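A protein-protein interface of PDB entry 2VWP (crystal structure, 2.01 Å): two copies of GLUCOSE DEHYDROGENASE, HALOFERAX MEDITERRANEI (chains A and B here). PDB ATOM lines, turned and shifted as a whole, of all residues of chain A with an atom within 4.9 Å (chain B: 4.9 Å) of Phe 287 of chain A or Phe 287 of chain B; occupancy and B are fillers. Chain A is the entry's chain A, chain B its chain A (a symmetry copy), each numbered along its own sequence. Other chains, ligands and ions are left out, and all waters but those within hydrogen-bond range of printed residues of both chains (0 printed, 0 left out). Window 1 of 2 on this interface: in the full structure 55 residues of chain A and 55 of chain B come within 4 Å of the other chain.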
ATOM      1  N   ALA A 256     -25.200   0.390 -15.718  1.00  0.00           N
ATOM      2  CA  ALA A 256     -24.054  -0.497 -15.966  1.00  0.00           C
ATOM      3  C   ALA A 256     -23.961  -1.597 -14.901  1.00  0.00           C
ATOM      4  O   ALA A 256     -23.812  -2.783 -15.230  1.00  0.00           O
ATOM      5  CB  ALA A 256     -22.753   0.296 -16.059  1.00  0.00           C
ATOM      6  N   ILE A 257     -24.104  -1.201 -13.634  1.00  0.00           N
ATOM      7  CA  ILE A 257     -24.064  -2.136 -12.495  1.00  0.00           C
ATOM      8  C   ILE A 257     -25.272  -3.058 -12.475  1.00  0.00           C
ATOM      9  O   ILE A 257     -25.141  -4.288 -12.421  1.00  0.00           O
ATOM     10  CB  ILE A 257     -23.986  -1.379 -11.117  1.00  0.00           C
ATOM     11  CG1 ILE A 257     -22.770  -0.427 -11.050  1.00  0.00           C
ATOM     12  CG2 ILE A 257     -24.038  -2.373  -9.937  1.00  0.00           C
ATOM     13  CD1 ILE A 257     -21.409  -1.075 -11.296  1.00  0.00           C
ATOM     14  N   VAL A 260     -26.242  -6.238 -14.901  1.00  0.00           N
ATOM     15  CA  VAL A 260     -25.720  -7.566 -14.543  1.00  0.00           C
ATOM     16  C   VAL A 260     -26.782  -8.402 -13.825  1.00  0.00           C
ATOM     17  O   VAL A 260     -26.975  -9.582 -14.148  1.00  0.00           O
ATOM     18  CB  VAL A 260     -24.391  -7.456 -13.715  1.00  0.00           C
ATOM     19  CG1 VAL A 260     -23.973  -8.813 -13.098  1.00  0.00           C
ATOM     20  CG2 VAL A 260     -23.273  -6.897 -14.607  1.00  0.00           C
ATOM     21  N   GLN A 261     -27.496  -7.774 -12.882  1.00  0.00           N
ATOM     22  CA  GLN A 261     -28.600  -8.442 -12.171  1.00  0.00           C
ATOM     23  C   GLN A 261     -29.814  -8.757 -13.045  1.00  0.00           C
ATOM     24  O   GLN A 261     -30.446  -9.787 -12.861  1.00  0.00           O
ATOM     25  CB  GLN A 261     -29.053  -7.629 -10.950  1.00  0.00           C
ATOM     26  CG  GLN A 261     -27.975  -7.320  -9.909  1.00  0.00           C
ATOM     27  CD  GLN A 261     -27.138  -8.530  -9.496  1.00  0.00           C
ATOM     28  OE1 GLN A 261     -25.903  -8.470  -9.503  1.00  0.00           O
ATOM     29  NE2 GLN A 261     -27.797  -9.624  -9.145  1.00  0.00           N
ATOM     30  N   ASP A 283     -22.907  -2.940  -4.318  1.00  0.00           N
ATOM     31  CA  ASP A 283     -22.588  -4.295  -3.888  1.00  0.00           C
ATOM     32  C   ASP A 283     -21.736  -4.942  -4.985  1.00  0.00           C
ATOM     33  O   ASP A 283     -22.269  -5.612  -5.886  1.00  0.00           O
ATOM     34  CB  ASP A 283     -23.863  -5.096  -3.633  1.00  0.00           C
ATOM     35  CG  ASP A 283     -23.605  -6.378  -2.848  1.00  0.00           C
ATOM     36  OD1 ASP A 283     -22.481  -6.928  -2.903  1.00  0.00           O
ATOM     37  OD2 ASP A 283     -24.549  -6.844  -2.180  1.00  0.00           O
ATOM     38  N   ALA A 284     -20.429  -4.682  -4.925  1.00  0.00           N
ATOM     39  CA  ALA A 284     -19.468  -5.212  -5.893  1.00  0.00           C
ATOM     40  C   ALA A 284     -19.360  -6.736  -5.824  1.00  0.00           C
ATOM     41  O   ALA A 284     -19.113  -7.393  -6.846  1.00  0.00           O
ATOM     42  CB  ALA A 284     -18.101  -4.567  -5.708  1.00  0.00           C
ATOM     43  N   GLY A 285     -19.539  -7.295  -4.628  1.00  0.00           N
ATOM     44  CA  GLY A 285     -19.500  -8.747  -4.451  1.00  0.00           C
ATOM     45  C   GLY A 285     -20.610  -9.443  -5.222  1.00  0.00           C
ATOM     46  O   GLY A 285     -20.389 -10.474  -5.863  1.00  0.00           O
ATOM     47  N   ALA A 286     -21.817  -8.895  -5.148  1.00  0.00           N
ATOM     48  CA  ALA A 286     -22.929  -9.464  -5.899  1.00  0.00           C
ATOM     49  C   ALA A 286     -22.734  -9.258  -7.407  1.00  0.00           C
ATOM     50  O   ALA A 286     -23.072 -10.136  -8.193  1.00  0.00           O
ATOM     51  CB  ALA A 286     -24.261  -8.878  -5.448  1.00  0.00           C
ATOM     52  N   PHE A 287     -22.221  -8.090  -7.787  1.00  0.00           N
ATOM     53  CA  PHE A 287     -21.889  -7.789  -9.177  1.00  0.00           C
ATOM     54  C   PHE A 287     -20.919  -8.848  -9.741  1.00  0.00           C
ATOM     55  O   PHE A 287     -21.214  -9.503 -10.751  1.00  0.00           O
ATOM     56  CB  PHE A 287     -21.300  -6.372  -9.285  1.00  0.00           C
ATOM     57  CG  PHE A 287     -20.724  -6.039 -10.652  1.00  0.00           C
ATOM     58  CD1 PHE A 287     -21.522  -5.464 -11.648  1.00  0.00           C
ATOM     59  CD2 PHE A 287     -19.378  -6.291 -10.937  1.00  0.00           C
ATOM     60  CE1 PHE A 287     -20.987  -5.152 -12.903  1.00  0.00           C
ATOM     61  CE2 PHE A 287     -18.836  -5.997 -12.202  1.00  0.00           C
ATOM     62  CZ  PHE A 287     -19.642  -5.420 -13.182  1.00  0.00           C
ATOM     63  N   HIS A 288     -19.778  -8.980  -9.063  1.00  0.00           N
ATOM     64  CA  HIS A 288     -18.701  -9.911  -9.366  1.00  0.00           C
ATOM     65  C   HIS A 288     -19.192 -11.362  -9.440  1.00  0.00           C
ATOM     66  O   HIS A 288     -19.026 -12.024 -10.472  1.00  0.00           O
ATOM     67  CB  HIS A 288     -17.609  -9.755  -8.285  1.00  0.00           C
ATOM     68  CG  HIS A 288     -16.306 -10.434  -8.596  1.00  0.00           C
ATOM     69  ND1 HIS A 288     -15.173 -10.231  -7.837  1.00  0.00           N
ATOM     70  CD2 HIS A 288     -15.945 -11.298  -9.578  1.00  0.00           C
ATOM     71  CE1 HIS A 288     -14.173 -10.937  -8.334  1.00  0.00           C
ATOM     72  NE2 HIS A 288     -14.615 -11.591  -9.393  1.00  0.00           N
ATOM     73  N   ARG A 289     -19.798 -11.864  -8.361  1.00  0.00           N
ATOM     74  CA  ARG A 289     -20.271 -13.259  -8.345  1.00  0.00           C
ATOM     75  C   ARG A 289     -21.273 -13.588  -9.468  1.00  0.00           C
ATOM     76  O   ARG A 289     -21.233 -14.684 -10.064  1.00  0.00           O
ATOM     77  CB  ARG A 289     -20.874 -13.608  -6.985  1.00  0.00           C
ATOM     78  CG  ARG A 289     -21.285 -15.068  -6.815  1.00  0.00           C
ATOM     79  CD  ARG A 289     -21.898 -15.335  -5.413  1.00  0.00           C
ATOM     80  NE  ARG A 289     -23.224 -14.725  -5.286  1.00  0.00           N
ATOM     81  CZ  ARG A 289     -23.491 -13.612  -4.602  1.00  0.00           C
ATOM     82  NH1 ARG A 289     -22.534 -12.963  -3.938  1.00  0.00           N
ATOM     83  NH2 ARG A 289     -24.731 -13.145  -4.585  1.00  0.00           N
ATOM     84  N   GLU A 290     -22.185 -12.655  -9.732  1.00  0.00           N
ATOM     85  CA  GLU A 290     -23.221 -12.864 -10.746  1.00  0.00           C
ATOM     86  C   GLU A 290     -22.628 -12.970 -12.151  1.00  0.00           C
ATOM     87  O   GLU A 290     -23.066 -13.802 -12.937  1.00  0.00           O
ATOM     88  CB  GLU A 290     -24.285 -11.754 -10.685  1.00  0.00           C
ATOM     89  CG  GLU A 290     -25.522 -12.016 -11.546  1.00  0.00           C
ATOM     90  CD  GLU A 290     -26.251 -13.301 -11.180  1.00  0.00           C
ATOM     91  OE1 GLU A 290     -26.044 -13.828 -10.061  1.00  0.00           O
ATOM     92  OE2 GLU A 290     -27.044 -13.784 -12.001  1.00  0.00           O
ATOM     93  N   MET A 291     -21.639 -12.118 -12.455  1.00  0.00           N
ATOM     94  CA  MET A 291     -20.880 -12.212 -13.709  1.00  0.00           C
ATOM     95  C   MET A 291     -20.295 -13.603 -13.911  1.00  0.00           C
ATOM     96  O   MET A 291     -20.375 -14.175 -15.000  1.00  0.00           O
ATOM     97  CB  MET A 291     -19.738 -11.201 -13.726  1.00  0.00           C
ATOM     98  CG  MET A 291     -20.153  -9.747 -13.845  1.00  0.00           C
ATOM     99  SD  MET A 291     -20.620  -9.297 -15.518  1.00  0.00           S
ATOM    100  CE  MET A 291     -19.035  -9.156 -16.331  1.00  0.00           C
ATOM    101  N   LEU A 298     -20.113  -8.039 -20.099  1.00  0.00           N
ATOM    102  CA  LEU A 298     -20.368  -6.640 -20.358  1.00  0.00           C
ATOM    103  C   LEU A 298     -19.370  -6.190 -21.404  1.00  0.00           C
ATOM    104  O   LEU A 298     -18.151  -6.437 -21.281  1.00  0.00           O
ATOM    105  CB  LEU A 298     -20.200  -5.815 -19.088  1.00  0.00           C
ATOM    106  CG  LEU A 298     -21.254  -5.873 -17.989  1.00  0.00           C
ATOM    107  CD1 LEU A 298     -20.788  -5.007 -16.786  1.00  0.00           C
ATOM    108  CD2 LEU A 298     -22.644  -5.419 -18.511  1.00  0.00           C
ATOM    109  N   ALA B 256     -12.680  -6.892  -9.620  1.00  0.00           N
ATOM    110  CA  ALA B 256     -13.635  -6.819 -10.736  1.00  0.00           C
ATOM    111  C   ALA B 256     -13.809  -5.375 -11.225  1.00  0.00           C
ATOM    112  O   ALA B 256     -13.742  -5.106 -12.434  1.00  0.00           O
ATOM    113  CB  ALA B 256     -14.977  -7.441 -10.356  1.00  0.00           C
ATOM    114  N   ILE B 257     -13.977  -4.450 -10.277  1.00  0.00           N
ATOM    115  CA  ILE B 257     -14.134  -3.016 -10.578  1.00  0.00           C
ATOM    116  C   ILE B 257     -12.852  -2.407 -11.123  1.00  0.00           C
ATOM    117  O   ILE B 257     -12.841  -1.782 -12.191  1.00  0.00           O
ATOM    118  CB  ILE B 257     -14.582  -2.197  -9.312  1.00  0.00           C
ATOM    119  CG1 ILE B 257     -15.893  -2.745  -8.704  1.00  0.00           C
ATOM    120  CG2 ILE B 257     -14.651  -0.687  -9.627  1.00  0.00           C
ATOM    121  CD1 ILE B 257     -17.086  -2.811  -9.655  1.00  0.00           C
ATOM    122  N   VAL B 260     -11.029  -2.857 -14.784  1.00  0.00           N
ATOM    123  CA  VAL B 260     -11.448  -1.969 -15.880  1.00  0.00           C
ATOM    124  C   VAL B 260     -10.460  -0.813 -16.063  1.00  0.00           C
ATOM    125  O   VAL B 260     -10.064  -0.500 -17.193  1.00  0.00           O
ATOM    126  CB  VAL B 260     -12.921  -1.466 -15.680  1.00  0.00           C
ATOM    127  CG1 VAL B 260     -13.288  -0.326 -16.662  1.00  0.00           C
ATOM    128  CG2 VAL B 260     -13.893  -2.645 -15.828  1.00  0.00           C
ATOM    129  N   GLN B 261     -10.036  -0.212 -14.944  1.00  0.00           N
ATOM    130  CA  GLN B 261      -9.027   0.861 -14.976  1.00  0.00           C
ATOM    131  C   GLN B 261      -7.631   0.402 -15.398  1.00  0.00           C
ATOM    132  O   GLN B 261      -6.930   1.137 -16.079  1.00  0.00           O
ATOM    133  CB  GLN B 261      -8.935   1.583 -13.623  1.00  0.00           C
ATOM    134  CG  GLN B 261     -10.231   2.205 -13.102  1.00  0.00           C
ATOM    135  CD  GLN B 261     -10.982   3.046 -14.134  1.00  0.00           C
ATOM    136  OE1 GLN B 261     -12.188   2.861 -14.337  1.00  0.00           O
ATOM    137  NE2 GLN B 261     -10.281   3.958 -14.789  1.00  0.00           N
ATOM    138  N   ASP B 283     -16.827   4.323  -7.797  1.00  0.00           N
ATOM    139  CA  ASP B 283     -17.059   5.312  -8.841  1.00  0.00           C
ATOM    140  C   ASP B 283     -17.585   4.569 -10.074  1.00  0.00           C
ATOM    141  O   ASP B 283     -16.802   4.176 -10.956  1.00  0.00           O
ATOM    142  CB  ASP B 283     -15.776   6.074  -9.161  1.00  0.00           C
ATOM    143  CG  ASP B 283     -16.030   7.343  -9.968  1.00  0.00           C
ATOM    144  OD1 ASP B 283     -17.044   7.424 -10.699  1.00  0.00           O
ATOM    145  OD2 ASP B 283     -15.193   8.262  -9.876  1.00  0.00           O
ATOM    146  N   ALA B 284     -18.899   4.336 -10.088  1.00  0.00           N
ATOM    147  CA  ALA B 284     -19.571   3.636 -11.184  1.00  0.00           C
ATOM    148  C   ALA B 284     -19.505   4.419 -12.496  1.00  0.00           C
ATOM    149  O   ALA B 284     -19.456   3.820 -13.580  1.00  0.00           O
ATOM    150  CB  ALA B 284     -21.014   3.319 -10.819  1.00  0.00           C
ATOM    151  N   GLY B 285     -19.506   5.747 -12.401  1.00  0.00           N
ATOM    152  CA  GLY B 285     -19.403   6.598 -13.588  1.00  0.00           C
ATOM    153  C   GLY B 285     -18.084   6.400 -14.315  1.00  0.00           C
ATOM    154  O   GLY B 285     -18.042   6.315 -15.545  1.00  0.00           O
ATOM    155  N   ALA B 286     -16.992   6.346 -13.561  1.00  0.00           N
ATOM    156  CA  ALA B 286     -15.690   6.104 -14.168  1.00  0.00           C
ATOM    157  C   ALA B 286     -15.597   4.674 -14.715  1.00  0.00           C
ATOM    158  O   ALA B 286     -15.002   4.457 -15.764  1.00  0.00           O
ATOM    159  CB  ALA B 286     -14.560   6.374 -13.183  1.00  0.00           C
ATOM    160  N   PHE B 287     -16.161   3.718 -13.979  1.00  0.00           N
ATOM    161  CA  PHE B 287     -16.236   2.327 -14.416  1.00  0.00           C
ATOM    162  C   PHE B 287     -16.935   2.230 -15.789  1.00  0.00           C
ATOM    163  O   PHE B 287     -16.363   1.708 -16.756  1.00  0.00           O
ATOM    164  CB  PHE B 287     -16.959   1.477 -13.357  1.00  0.00           C
ATOM    165  CG  PHE B 287     -17.280   0.061 -13.807  1.00  0.00           C
ATOM    166  CD1 PHE B 287     -16.371  -0.983 -13.598  1.00  0.00           C
ATOM    167  CD2 PHE B 287     -18.498  -0.228 -14.429  1.00  0.00           C
ATOM    168  CE1 PHE B 287     -16.673  -2.288 -14.007  1.00  0.00           C
ATOM    169  CE2 PHE B 287     -18.803  -1.533 -14.860  1.00  0.00           C
ATOM    170  CZ  PHE B 287     -17.891  -2.564 -14.640  1.00  0.00           C
ATOM    171  N   HIS B 288     -18.165   2.744 -15.828  1.00  0.00           N
ATOM    172  CA  HIS B 288     -19.036   2.800 -16.993  1.00  0.00           C
ATOM    173  C   HIS B 288     -18.368   3.496 -18.184  1.00  0.00           C
ATOM    174  O   HIS B 288     -18.238   2.900 -19.262  1.00  0.00           O
ATOM    175  CB  HIS B 288     -20.336   3.530 -16.589  1.00  0.00           C
ATOM    176  CG  HIS B 288     -21.457   3.429 -17.585  1.00  0.00           C
ATOM    177  ND1 HIS B 288     -22.736   3.852 -17.294  1.00  0.00           N
ATOM    178  CD2 HIS B 288     -21.502   2.951 -18.854  1.00  0.00           C
ATOM    179  CE1 HIS B 288     -23.520   3.640 -18.337  1.00  0.00           C
ATOM    180  NE2 HIS B 288     -22.796   3.091 -19.294  1.00  0.00           N
ATOM    181  N   ARG B 289     -17.938   4.748 -18.006  1.00  0.00           N
ATOM    182  CA  ARG B 289     -17.312   5.493 -19.112  1.00  0.00           C
ATOM    183  C   ARG B 289     -16.070   4.799 -19.703  1.00  0.00           C
ATOM    184  O   ARG B 289     -15.854   4.807 -20.932  1.00  0.00           O
ATOM    185  CB  ARG B 289     -16.962   6.914 -18.675  1.00  0.00           C
ATOM    186  CG  ARG B 289     -16.419   7.816 -19.779  1.00  0.00           C
ATOM    187  CD  ARG B 289     -16.077   9.235 -19.249  1.00  0.00           C
ATOM    188  NE  ARG B 289     -14.889   9.212 -18.392  1.00  0.00           N
ATOM    189  CZ  ARG B 289     -14.904   9.301 -17.062  1.00  0.00           C
ATOM    190  NH1 ARG B 289     -16.048   9.447 -16.392  1.00  0.00           N
ATOM    191  NH2 ARG B 289     -13.760   9.241 -16.397  1.00  0.00           N
ATOM    192  N   GLU B 290     -15.244   4.230 -18.828  1.00  0.00           N
ATOM    193  CA  GLU B 290     -14.005   3.579 -19.260  1.00  0.00           C
ATOM    194  C   GLU B 290     -14.282   2.339 -20.111  1.00  0.00           C
ATOM    195  O   GLU B 290     -13.595   2.112 -21.100  1.00  0.00           O
ATOM    196  CB  GLU B 290     -13.119   3.225 -18.052  1.00  0.00           C
ATOM    197  CG  GLU B 290     -11.710   2.754 -18.418  1.00  0.00           C
ATOM    198  CD  GLU B 290     -10.921   3.782 -19.218  1.00  0.00           C
ATOM    199  OE1 GLU B 290     -11.285   4.981 -19.209  1.00  0.00           O
ATOM    200  OE2 GLU B 290      -9.923   3.399 -19.848  1.00  0.00           O
ATOM    201  N   MET B 291     -15.284   1.544 -19.711  1.00  0.00           N
ATOM    202  CA  MET B 291     -15.755   0.409 -20.517  1.00  0.00           C
ATOM    203  C   MET B 291     -16.112   0.835 -21.934  1.00  0.00           C
ATOM    204  O   MET B 291     -15.744   0.176 -22.909  1.00  0.00           O
ATOM    205  CB  MET B 291     -16.983  -0.232 -19.881  1.00  0.00           C
ATOM    206  CG  MET B 291     -16.733  -0.987 -18.589  1.00  0.00           C
ATOM    207  SD  MET B 291     -15.993  -2.598 -18.864  1.00  0.00           S
ATOM    208  CE  MET B 291     -17.384  -3.564 -19.434  1.00  0.00           C
ATOM    209  N   LEU B 298     -15.704  -7.240 -19.957  1.00  0.00           N
ATOM    210  CA  LEU B 298     -15.574  -8.109 -18.809  1.00  0.00           C
ATOM    211  C   LEU B 298     -16.385  -9.356 -19.098  1.00  0.00           C
ATOM    212  O   LEU B 298     -17.564  -9.277 -19.505  1.00  0.00           O
ATOM    213  CB  LEU B 298     -16.096  -7.427 -17.551  1.00  0.00           C
ATOM    214  CG  LEU B 298     -15.289  -6.317 -16.887  1.00  0.00           C
ATOM    215  CD1 LEU B 298     -16.092  -5.750 -15.685  1.00  0.00           C
ATOM    216  CD2 LEU B 298     -13.888  -6.821 -16.448  1.00  0.00           C
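Of the 14 printed residues of chain B, 5 touch a printed residue of chain A. Among the printed residues, no Asp or Glu carboxylate lies within 4 Å of a Lys or Arg side-chain nitrogen of the other chain.
Ala 256 of chain A touches His 288 of chain B. CZ of Phe 287 of chain A touches CZ of Phe 287 of chain B, at 3.7 Å. Ala 256 of chain B touches His 288 of chain A (CB to CG, 3.7 Å). CE of Met 291 of chain A touches O of Leu 298 of chain B (3.5 Å). Leu 298 of chain A touches Met 291 of chain B.
Printed residues of chain B within 4 Å of Ala 256 of chain A: His 288 (3.7 Å). Of chain B, only Phe 287 comes within 4 Å of Phe 287 of chain A. Printed residues of chain B within 4 Å of Leu 298 of chain A: Met 291 (3.5 Å) and Leu 298 (2.9 Å). Of the printed residues of chain A, Phe 287 of chain B touches Phe 287. Of the printed residues of chain A, His 288 of chain B touches Ala 256 (3.7 Å). Printed residues of chain A within 4 Å of Met 291 of chain B: Leu 298.
The backbone carbonyl oxygen (O) of Leu 298 of chain B is in hydrogen-bond range of the backbone NH (N) of Leu 298 of chain A, 2.9 Å away.
Ala 256 of chain A touches His 288 of chain B, and with the chains exchanged His 288 of chain A touches Ala 256 of chain B. Phe 287 of chain B touches its own counterpart, Phe 287 of chain A. Met 291 of chain A touches Leu 298 of chain B, and with the chains exchanged Leu 298 of chain A touches Met 291 of chain B. Leu 298 of chain B touches its own counterpart, Leu 298 of chain A. Positions printed for both chains: 256, 257, 260, 261, 283, 284, 285, 286, 287, 288, 289, 290, 291 and 298. Of the 6 pairs that touch across the chains among the printed residues, 6 have their exchanged pair printed and touching as well.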
